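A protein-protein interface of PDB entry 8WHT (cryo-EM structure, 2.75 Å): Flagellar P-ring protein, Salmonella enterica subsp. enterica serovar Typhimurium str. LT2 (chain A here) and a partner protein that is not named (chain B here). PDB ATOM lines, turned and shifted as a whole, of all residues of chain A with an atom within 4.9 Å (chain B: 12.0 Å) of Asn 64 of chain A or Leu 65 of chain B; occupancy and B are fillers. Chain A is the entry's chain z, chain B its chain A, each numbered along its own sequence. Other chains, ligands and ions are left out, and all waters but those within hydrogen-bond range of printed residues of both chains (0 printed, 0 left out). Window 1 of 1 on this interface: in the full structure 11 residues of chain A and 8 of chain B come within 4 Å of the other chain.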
ATOM      1  N   GLN A  60     -23.334 -17.773  26.584  1.00  0.00           N
ATOM      2  CA  GLN A  60     -22.843 -19.071  26.136  1.00  0.00           C
ATOM      3  C   GLN A  60     -23.389 -19.421  24.756  1.00  0.00           C
ATOM      4  O   GLN A  60     -22.645 -19.863  23.872  1.00  0.00           O
ATOM      5  CB  GLN A  60     -23.214 -20.148  27.152  1.00  0.00           C
ATOM      6  CG  GLN A  60     -22.560 -21.491  26.895  1.00  0.00           C
ATOM      7  CD  GLN A  60     -23.010 -22.549  27.876  1.00  0.00           C
ATOM      8  OE1 GLN A  60     -23.737 -22.261  28.825  1.00  0.00           O
ATOM      9  NE2 GLN A  60     -22.576 -23.783  27.657  1.00  0.00           N
ATOM     10  N   THR A  61     -24.687 -19.206  24.540  1.00  0.00           N
ATOM     11  CA  THR A  61     -25.284 -19.530  23.252  1.00  0.00           C
ATOM     12  C   THR A  61     -24.909 -18.520  22.174  1.00  0.00           C
ATOM     13  O   THR A  61     -24.813 -18.890  20.998  1.00  0.00           O
ATOM     14  CB  THR A  61     -26.802 -19.631  23.388  1.00  0.00           C
ATOM     15  OG1 THR A  61     -27.313 -18.431  23.978  1.00  0.00           O
ATOM     16  CG2 THR A  61     -27.165 -20.811  24.265  1.00  0.00           C
ATOM     17  N   LEU A  62     -24.669 -17.258  22.542  1.00  0.00           N
ATOM     18  CA  LEU A  62     -24.136 -16.315  21.566  1.00  0.00           C
ATOM     19  C   LEU A  62     -22.746 -16.734  21.107  1.00  0.00           C
ATOM     20  O   LEU A  62     -22.428 -16.660  19.912  1.00  0.00           O
ATOM     21  CB  LEU A  62     -24.105 -14.903  22.148  1.00  0.00           C
ATOM     22  CG  LEU A  62     -23.939 -13.792  21.109  1.00  0.00           C
ATOM     23  CD1 LEU A  62     -25.290 -13.222  20.707  1.00  0.00           C
ATOM     24  CD2 LEU A  62     -23.021 -12.696  21.620  1.00  0.00           C
ATOM     25  N   ASN A  63     -21.903 -17.179  22.042  1.00  0.00           N
ATOM     26  CA  ASN A  63     -20.590 -17.695  21.672  1.00  0.00           C
ATOM     27  C   ASN A  63     -20.712 -18.944  20.812  1.00  0.00           C
ATOM     28  O   ASN A  63     -19.928 -19.138  19.878  1.00  0.00           O
ATOM     29  CB  ASN A  63     -19.767 -17.986  22.926  1.00  0.00           C
ATOM     30  CG  ASN A  63     -19.234 -16.729  23.578  1.00  0.00           C
ATOM     31  OD1 ASN A  63     -19.192 -16.620  24.802  1.00  0.00           O
ATOM     32  ND2 ASN A  63     -18.820 -15.769  22.758  1.00  0.00           N
ATOM     33  N   ASN A  64     -21.682 -19.806  21.119  1.00  0.00           N
ATOM     34  CA  ASN A  64     -21.919 -20.985  20.288  1.00  0.00           C
ATOM     35  C   ASN A  64     -22.275 -20.588  18.859  1.00  0.00           C
ATOM     36  O   ASN A  64     -21.751 -21.154  17.894  1.00  0.00           O
ATOM     37  CB  ASN A  64     -23.027 -21.841  20.899  1.00  0.00           C
ATOM     38  CG  ASN A  64     -22.515 -22.788  21.961  1.00  0.00           C
ATOM     39  OD1 ASN A  64     -21.526 -23.488  21.759  1.00  0.00           O
ATOM     40  ND2 ASN A  64     -23.188 -22.814  23.104  1.00  0.00           N
ATOM     41  N   MET A  65     -23.170 -19.609  18.711  1.00  0.00           N
ATOM     42  CA  MET A  65     -23.566 -19.153  17.381  1.00  0.00           C
ATOM     43  C   MET A  65     -22.386 -18.543  16.635  1.00  0.00           C
ATOM     44  O   MET A  65     -22.190 -18.800  15.441  1.00  0.00           O
ATOM     45  CB  MET A  65     -24.712 -18.146  17.493  1.00  0.00           C
ATOM     46  CG  MET A  65     -24.859 -17.229  16.290  1.00  0.00           C
ATOM     47  SD  MET A  65     -26.283 -16.134  16.417  1.00  0.00           S
ATOM     48  CE  MET A  65     -25.569 -14.753  17.302  1.00  0.00           C
ATOM     49  N   LEU A  66     -21.589 -17.726  17.326  1.00  0.00           N
ATOM     50  CA  LEU A  66     -20.423 -17.119  16.689  1.00  0.00           C
ATOM     51  C   LEU A  66     -19.409 -18.174  16.265  1.00  0.00           C
ATOM     52  O   LEU A  66     -18.821 -18.080  15.182  1.00  0.00           O
ATOM     53  CB  LEU A  66     -19.780 -16.101  17.631  1.00  0.00           C
ATOM     54  CG  LEU A  66     -20.554 -14.796  17.819  1.00  0.00           C
ATOM     55  CD1 LEU A  66     -19.857 -13.893  18.822  1.00  0.00           C
ATOM     56  CD2 LEU A  66     -20.736 -14.083  16.489  1.00  0.00           C
ATOM     57  N   SER A  67     -19.188 -19.186  17.108  1.00  0.00           N
ATOM     58  CA  SER A  67     -18.282 -20.272  16.752  1.00  0.00           C
ATOM     59  C   SER A  67     -18.794 -21.039  15.542  1.00  0.00           C
ATOM     60  O   SER A  67     -18.011 -21.434  14.671  1.00  0.00           O
ATOM     61  CB  SER A  67     -18.099 -21.210  17.945  1.00  0.00           C
ATOM     62  OG  SER A  67     -17.171 -22.237  17.650  1.00  0.00           O
ATOM     63  N   GLN A  68     -20.106 -21.268  15.479  1.00  0.00           N
ATOM     64  CA  GLN A  68     -20.685 -21.910  14.305  1.00  0.00           C
ATOM     65  C   GLN A  68     -20.481 -21.055  13.059  1.00  0.00           C
ATOM     66  O   GLN A  68     -20.235 -21.582  11.969  1.00  0.00           O
ATOM     67  CB  GLN A  68     -22.169 -22.186  14.536  1.00  0.00           C
ATOM     68  CG  GLN A  68     -22.863 -22.884  13.381  1.00  0.00           C
ATOM     69  CD  GLN A  68     -22.289 -24.257  13.104  1.00  0.00           C
ATOM     70  OE1 GLN A  68     -22.313 -25.136  13.964  1.00  0.00           O
ATOM     71  NE2 GLN A  68     -21.763 -24.448  11.902  1.00  0.00           N
ATOM     72  N   MET A 123     -32.341 -17.878  13.902  1.00  0.00           N
ATOM     73  CA  MET A 123     -32.699 -19.237  13.515  1.00  0.00           C
ATOM     74  C   MET A 123     -32.900 -20.118  14.740  1.00  0.00           C
ATOM     75  O   MET A 123     -31.965 -20.361  15.508  1.00  0.00           O
ATOM     76  CB  MET A 123     -31.611 -19.820  12.613  1.00  0.00           C
ATOM     77  CG  MET A 123     -32.007 -21.117  11.930  1.00  0.00           C
ATOM     78  SD  MET A 123     -33.721 -21.094  11.383  1.00  0.00           S
ATOM     79  CE  MET A 123     -33.527 -20.573   9.683  1.00  0.00           C
ATOM     80  N   TYR B  60     -22.168 -30.579   4.964  1.00  0.00           N
ATOM     81  CA  TYR B  60     -22.022 -31.279   6.232  1.00  0.00           C
ATOM     82  C   TYR B  60     -23.349 -31.418   6.972  1.00  0.00           C
ATOM     83  O   TYR B  60     -23.357 -31.740   8.164  1.00  0.00           O
ATOM     84  CB  TYR B  60     -20.988 -30.572   7.109  1.00  0.00           C
ATOM     85  CG  TYR B  60     -19.648 -30.390   6.432  1.00  0.00           C
ATOM     86  CD1 TYR B  60     -19.027 -31.450   5.788  1.00  0.00           C
ATOM     87  CD2 TYR B  60     -19.004 -29.161   6.438  1.00  0.00           C
ATOM     88  CE1 TYR B  60     -17.802 -31.292   5.167  1.00  0.00           C
ATOM     89  CE2 TYR B  60     -17.779 -28.992   5.821  1.00  0.00           C
ATOM     90  CZ  TYR B  60     -17.183 -30.061   5.186  1.00  0.00           C
ATOM     91  OH  TYR B  60     -15.964 -29.903   4.568  1.00  0.00           O
ATOM     92  N   GLY B  61     -24.464 -31.174   6.290  1.00  0.00           N
ATOM     93  CA  GLY B  61     -25.769 -31.353   6.884  1.00  0.00           C
ATOM     94  C   GLY B  61     -26.172 -30.201   7.785  1.00  0.00           C
ATOM     95  O   GLY B  61     -25.483 -29.186   7.916  1.00  0.00           O
ATOM     96  N   TYR B  62     -27.329 -30.380   8.419  1.00  0.00           N
ATOM     97  CA  TYR B  62     -27.855 -29.371   9.326  1.00  0.00           C
ATOM     98  C   TYR B  62     -26.970 -29.247  10.560  1.00  0.00           C
ATOM     99  O   TYR B  62     -26.519 -30.249  11.122  1.00  0.00           O
ATOM    100  CB  TYR B  62     -29.287 -29.730   9.727  1.00  0.00           C
ATOM    101  CG  TYR B  62     -29.848 -28.909  10.865  1.00  0.00           C
ATOM    102  CD1 TYR B  62     -29.861 -29.403  12.162  1.00  0.00           C
ATOM    103  CD2 TYR B  62     -30.365 -27.641  10.643  1.00  0.00           C
ATOM    104  CE1 TYR B  62     -30.373 -28.659  13.203  1.00  0.00           C
ATOM    105  CE2 TYR B  62     -30.879 -26.890  11.680  1.00  0.00           C
ATOM    106  CZ  TYR B  62     -30.880 -27.405  12.957  1.00  0.00           C
ATOM    107  OH  TYR B  62     -31.391 -26.660  13.993  1.00  0.00           O
ATOM    108  N   GLN B  63     -26.719 -28.007  10.976  1.00  0.00           N
ATOM    109  CA  GLN B  63     -25.900 -27.726  12.150  1.00  0.00           C
ATOM    110  C   GLN B  63     -26.640 -26.727  13.027  1.00  0.00           C
ATOM    111  O   GLN B  63     -26.937 -25.605  12.568  1.00  0.00           O
ATOM    112  CB  GLN B  63     -24.524 -27.193  11.743  1.00  0.00           C
ATOM    113  CG  GLN B  63     -23.501 -28.283  11.467  1.00  0.00           C
ATOM    114  CD  GLN B  63     -22.527 -27.905  10.370  1.00  0.00           C
ATOM    115  OE1 GLN B  63     -22.634 -28.380   9.241  1.00  0.00           O
ATOM    116  NE2 GLN B  63     -21.567 -27.050  10.699  1.00  0.00           N
ATOM    117  N   PRO B  64     -26.970 -27.077  14.269  1.00  0.00           N
ATOM    118  CA  PRO B  64     -27.655 -26.124  15.146  1.00  0.00           C
ATOM    119  C   PRO B  64     -26.795 -24.901  15.427  1.00  0.00           C
ATOM    120  O   PRO B  64     -25.566 -24.976  15.490  1.00  0.00           O
ATOM    121  CB  PRO B  64     -27.909 -26.934  16.422  1.00  0.00           C
ATOM    122  CG  PRO B  64     -27.854 -28.361  15.983  1.00  0.00           C
ATOM    123  CD  PRO B  64     -26.844 -28.408  14.884  1.00  0.00           C
ATOM    124  N   LEU B  65     -27.463 -23.762  15.601  1.00  0.00           N
ATOM    125  CA  LEU B  65     -26.779 -22.488  15.785  1.00  0.00           C
ATOM    126  C   LEU B  65     -26.414 -22.229  17.243  1.00  0.00           C
ATOM    127  O   LEU B  65     -25.258 -21.926  17.550  1.00  0.00           O
ATOM    128  CB  LEU B  65     -27.654 -21.351  15.250  1.00  0.00           C
ATOM    129  CG  LEU B  65     -26.946 -20.197  14.539  1.00  0.00           C
ATOM    130  CD1 LEU B  65     -26.292 -20.677  13.256  1.00  0.00           C
ATOM    131  CD2 LEU B  65     -27.926 -19.074  14.256  1.00  0.00           C
ATOM    132  N   PHE B  66     -27.383 -22.342  18.152  1.00  0.00           N
ATOM    133  CA  PHE B  66     -27.158 -22.007  19.552  1.00  0.00           C
ATOM    134  C   PHE B  66     -26.835 -23.209  20.427  1.00  0.00           C
ATOM    135  O   PHE B  66     -26.430 -23.021  21.579  1.00  0.00           O
ATOM    136  CB  PHE B  66     -28.383 -21.289  20.131  1.00  0.00           C
ATOM    137  CG  PHE B  66     -28.855 -20.130  19.302  1.00  0.00           C
ATOM    138  CD1 PHE B  66     -28.052 -19.018  19.123  1.00  0.00           C
ATOM    139  CD2 PHE B  66     -30.102 -20.153  18.703  1.00  0.00           C
ATOM    140  CE1 PHE B  66     -28.482 -17.952  18.360  1.00  0.00           C
ATOM    141  CE2 PHE B  66     -30.537 -19.091  17.941  1.00  0.00           C
ATOM    142  CZ  PHE B  66     -29.727 -17.988  17.769  1.00  0.00           C
ATOM    143  N   GLU B  67     -27.002 -24.428  19.923  1.00  0.00           N
ATOM    144  CA  GLU B  67     -26.712 -25.607  20.727  1.00  0.00           C
ATOM    145  C   GLU B  67     -25.209 -25.791  20.894  1.00  0.00           C
ATOM    146  O   GLU B  67     -24.424 -25.487  19.991  1.00  0.00           O
ATOM    147  CB  GLU B  67     -27.330 -26.853  20.096  1.00  0.00           C
ATOM    148  CG  GLU B  67     -28.826 -26.982  20.323  1.00  0.00           C
ATOM    149  CD  GLU B  67     -29.500 -27.871  19.299  1.00  0.00           C
ATOM    150  OE1 GLU B  67     -30.492 -27.426  18.685  1.00  0.00           O
ATOM    151  OE2 GLU B  67     -29.037 -29.015  19.109  1.00  0.00           O
ATOM    152  N   ASP B  68     -24.815 -26.285  22.065  1.00  0.00           N
ATOM    153  CA  ASP B  68     -23.410 -26.550  22.341  1.00  0.00           C
ATOM    154  C   ASP B  68     -22.871 -27.605  21.382  1.00  0.00           C
ATOM    155  O   ASP B  68     -23.573 -28.552  21.019  1.00  0.00           O
ATOM    156  CB  ASP B  68     -23.238 -27.015  23.786  1.00  0.00           C
ATOM    157  CG  ASP B  68     -23.410 -25.890  24.786  1.00  0.00           C
ATOM    158  OD1 ASP B  68     -23.240 -26.139  25.995  1.00  0.00           O
ATOM    159  OD2 ASP B  68     -23.714 -24.756  24.363  1.00  0.00           O
ATOM    160  N   ARG B  69     -21.618 -27.437  20.970  1.00  0.00           N
ATOM    161  CA  ARG B  69     -21.001 -28.353  20.015  1.00  0.00           C
ATOM    162  C   ARG B  69     -20.748 -29.691  20.700  1.00  0.00           C
ATOM    163  O   ARG B  69     -19.903 -29.804  21.591  1.00  0.00           O
ATOM    164  CB  ARG B  69     -19.716 -27.762  19.447  1.00  0.00           C
ATOM    165  CG  ARG B  69     -18.761 -27.172  20.469  1.00  0.00           C
ATOM    166  CD  ARG B  69     -17.496 -26.673  19.791  1.00  0.00           C
ATOM    167  NE  ARG B  69     -16.484 -26.259  20.755  1.00  0.00           N
ATOM    168  CZ  ARG B  69     -15.380 -26.945  21.016  1.00  0.00           C
ATOM    169  NH1 ARG B  69     -15.112 -28.084  20.400  1.00  0.00           N
ATOM    170  NH2 ARG B  69     -14.522 -26.475  21.918  1.00  0.00           N
ATOM    171  N   ARG B  70     -21.496 -30.708  20.292  1.00  0.00           N
ATOM    172  CA  ARG B  70     -21.400 -32.055  20.821  1.00  0.00           C
ATOM    173  C   ARG B  70     -21.087 -33.038  19.701  1.00  0.00           C
ATOM    174  O   ARG B  70     -21.453 -32.805  18.544  1.00  0.00           O
ATOM    175  CB  ARG B  70     -22.709 -32.478  21.500  1.00  0.00           C
ATOM    176  CG  ARG B  70     -22.889 -31.986  22.924  1.00  0.00           C
ATOM    177  CD  ARG B  70     -24.250 -32.406  23.458  1.00  0.00           C
ATOM    178  NE  ARG B  70     -24.633 -31.682  24.664  1.00  0.00           N
ATOM    179  CZ  ARG B  70     -25.860 -31.667  25.168  1.00  0.00           C
ATOM    180  NH1 ARG B  70     -26.853 -32.323  24.590  1.00  0.00           N
ATOM    181  NH2 ARG B  70     -26.097 -30.979  26.281  1.00  0.00           N
ATOM    182  N   PRO B  71     -20.406 -34.141  19.999  1.00  0.00           N
ATOM    183  CA  PRO B  71     -20.289 -35.211  19.004  1.00  0.00           C
ATOM    184  C   PRO B  71     -21.645 -35.853  18.766  1.00  0.00           C
ATOM    185  O   PRO B  71     -22.409 -36.101  19.702  1.00  0.00           O
ATOM    186  CB  PRO B  71     -19.300 -36.193  19.644  1.00  0.00           C
ATOM    187  CG  PRO B  71     -19.340 -35.893  21.100  1.00  0.00           C
ATOM    188  CD  PRO B  71     -19.672 -34.443  21.240  1.00  0.00           C
ATOM    189  N   ARG B  72     -21.953 -36.105  17.494  1.00  0.00           N
ATOM    190  CA  ARG B  72     -23.271 -36.611  17.135  1.00  0.00           C
ATOM    191  C   ARG B  72     -23.189 -37.830  16.226  1.00  0.00           C
ATOM    192  O   ARG B  72     -24.081 -38.685  16.247  1.00  0.00           O
ATOM    193  CB  ARG B  72     -24.093 -35.509  16.461  1.00  0.00           C
ATOM    194  CG  ARG B  72     -24.333 -34.294  17.337  1.00  0.00           C
ATOM    195  CD  ARG B  72     -25.002 -33.173  16.567  1.00  0.00           C
ATOM    196  NE  ARG B  72     -24.633 -31.865  17.095  1.00  0.00           N
ATOM    197  CZ  ARG B  72     -25.331 -31.201  18.005  1.00  0.00           C
ATOM    198  NH1 ARG B  72     -26.450 -31.691  18.511  1.00  0.00           N
ATOM    199  NH2 ARG B  72     -24.894 -30.015  18.419  1.00  0.00           N
ATOM    200  N   ILE B 189     -21.705 -34.061  28.497  1.00  0.00           N
ATOM    201  CA  ILE B 189     -20.651 -33.294  27.844  1.00  0.00           C
ATOM    202  C   ILE B 189     -20.872 -31.811  28.110  1.00  0.00           C
ATOM    203  O   ILE B 189     -21.991 -31.301  27.988  1.00  0.00           O
ATOM    204  CB  ILE B 189     -20.618 -33.601  26.337  1.00  0.00           C
ATOM    205  CG1 ILE B 189     -20.346 -35.087  26.104  1.00  0.00           C
ATOM    206  CG2 ILE B 189     -19.566 -32.755  25.640  1.00  0.00           C
ATOM    207  CD1 ILE B 189     -20.822 -35.592  24.762  1.00  0.00           C
ATOM    208  N   SER B 190     -19.799 -31.113  28.471  1.00  0.00           N
ATOM    209  CA  SER B 190     -19.881 -29.710  28.844  1.00  0.00           C
ATOM    210  C   SER B 190     -19.970 -28.828  27.600  1.00  0.00           C
ATOM    211  O   SER B 190     -19.954 -29.301  26.462  1.00  0.00           O
ATOM    212  CB  SER B 190     -18.680 -29.319  29.701  1.00  0.00           C
ATOM    213  OG  SER B 190     -17.504 -29.226  28.916  1.00  0.00           O
ATOM    214  N   GLY B 191     -20.061 -27.515  27.828  1.00  0.00           N
ATOM    215  CA  GLY B 191     -20.161 -26.570  26.730  1.00  0.00           C
ATOM    216  C   GLY B 191     -18.900 -26.445  25.906  1.00  0.00           C
ATOM    217  O   GLY B 191     -18.968 -26.021  24.748  1.00  0.00           O
ATOM    218  N   SER B 192     -17.749 -26.802  26.475  1.00  0.00           N
ATOM    219  CA  SER B 192     -16.481 -26.782  25.765  1.00  0.00           C
ATOM    220  C   SER B 192     -16.115 -28.143  25.184  1.00  0.00           C
ATOM    221  O   SER B 192     -14.928 -28.417  24.974  1.00  0.00           O
ATOM    222  CB  SER B 192     -15.367 -26.289  26.691  1.00  0.00           C
ATOM    223  OG  SER B 192     -15.165 -27.187  27.767  1.00  0.00           O
ATOM    224  N   ASN B 193     -17.110 -28.994  24.927  1.00  0.00           N
ATOM    225  CA  ASN B 193     -16.900 -30.324  24.355  1.00  0.00           C
ATOM    226  C   ASN B 193     -15.937 -31.148  25.207  1.00  0.00           C
ATOM    227  O   ASN B 193     -14.965 -31.722  24.714  1.00  0.00           O
ATOM    228  CB  ASN B 193     -16.413 -30.231  22.907  1.00  0.00           C
ATOM    229  CG  ASN B 193     -16.717 -31.481  22.112  1.00  0.00           C
ATOM    230  OD1 ASN B 193     -17.795 -32.058  22.235  1.00  0.00           O
ATOM    231  ND2 ASN B 193     -15.766 -31.909  21.293  1.00  0.00           N
ATOM    232  N   SER B 194     -16.218 -31.203  26.506  1.00  0.00           N
ATOM    233  CA  SER B 194     -15.384 -31.935  27.443  1.00  0.00           C
ATOM    234  C   SER B 194     -16.263 -32.711  28.410  1.00  0.00           C
ATOM    235  O   SER B 194     -17.352 -32.265  28.780  1.00  0.00           O
ATOM    236  CB  SER B 194     -14.454 -30.994  28.217  1.00  0.00           C
ATOM    237  OG  SER B 194     -13.280 -31.667  28.631  1.00  0.00           O
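Hydrophobic or aromatic side chains of chain B within 4 Å of the printed part of chain A: Phe 66.
Of the 10 printed residues of chain A, 6 touch a printed residue of chain B.
Among the printed residues, 12 pairs touch across the chains.
O of Leu 65 of chain B sits close to N of Met 65 of chain A (3.3 Å).
ND2 of Asn 64 of chain A sits close to OD2 of Asp 68 of chain B (2.4 Å).
NE2 of Gln 60 of chain A is in hydrogen-bond range of OD1 of Asp 68 of chain B (3.0 Å).
NE2 of Gln 63 of chain B sits close to NE2 of Gln 68 of chain A (2.9 Å).
NE2 of Gln 60 of chain A touches CA of Gly 191 of chain B, 3.8 Å away.
Thr 61 of chain A touches Phe 66 of chain B (CG2 to O, 3.6 Å).
C of Asn 64 of chain A touches O of Leu 65 of chain B (3.5 Å).
Phe 66 of chain B touches Asn 64 of chain A.
Glu 67 of chain B touches Asn 64 of chain A (O to CG, 3.8 Å).
Phe 66 of chain B touches Met 65 of chain A.
Gln 68 of chain A touches Pro 64 of chain B.
O of Met 123 of chain A touches CE2 of Phe 66 of chain B, at 3.1 Å.
Asn 64 of chain A touches just these residues of chain B: Leu 65, Phe 66, Glu 67 and Asp 68.
Of chain A, only Asn 64 (3.5 Å) and Met 65 (3.3 Å) come within 4 Å of Leu 65 of chain B.
Of the printed residues of chain B, Thr 61 of chain A touches Phe 66 (3.6 Å).
No residue of chain B comes within 4 Å of Asn 63 of chain A.
Leu 66 of chain A touches none of the printed residues of chain B.
No residue of chain B comes within 4 Å of Ser 67 of chain A.
Printed residues of chain B within 4 Å of Gln 68 of chain A: Gln 63 and Pro 64.
Of the printed residues of chain A, Pro 64 of chain B touches Gln 68 (3.6 Å).
Of the printed residues of chain A, Phe 66 of chain B touches Thr 61, Asn 64, Met 65 and Met 123.
Of the printed residues of chain A, Gly 191 of chain B touches Gln 60.
Of the printed residues of chain A, Glu 67 of chain B touches Asn 64.
Asn 193 of chain B touches none of the printed residues of chain A.
Ser 190 of chain B touches none of the printed residues of chain A.
The backbone carbonyl oxygen (O) of Gly 61 of chain B lies close to the side-chain amide oxygen (OE1) of Gln 63 of chain B.
The backbone carbonyl oxygen (O) of Asp 68 of chain B sits at hydrogen-bond distance from the guanidinium group (NH2) of Arg 72 of chain B (3.3 Å).
The side-chain carboxylate of Glu 67 of chain B is in salt-bridge range of the guanidinium group of Arg 72 of chain B (3.8 Å).
The backbone carbonyl oxygen (O) of Gln 60 of chain A lies within hydrogen-bond range of the side-chain amide nitrogen (ND2) of Asn 64 of chain A (3.1 Å).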
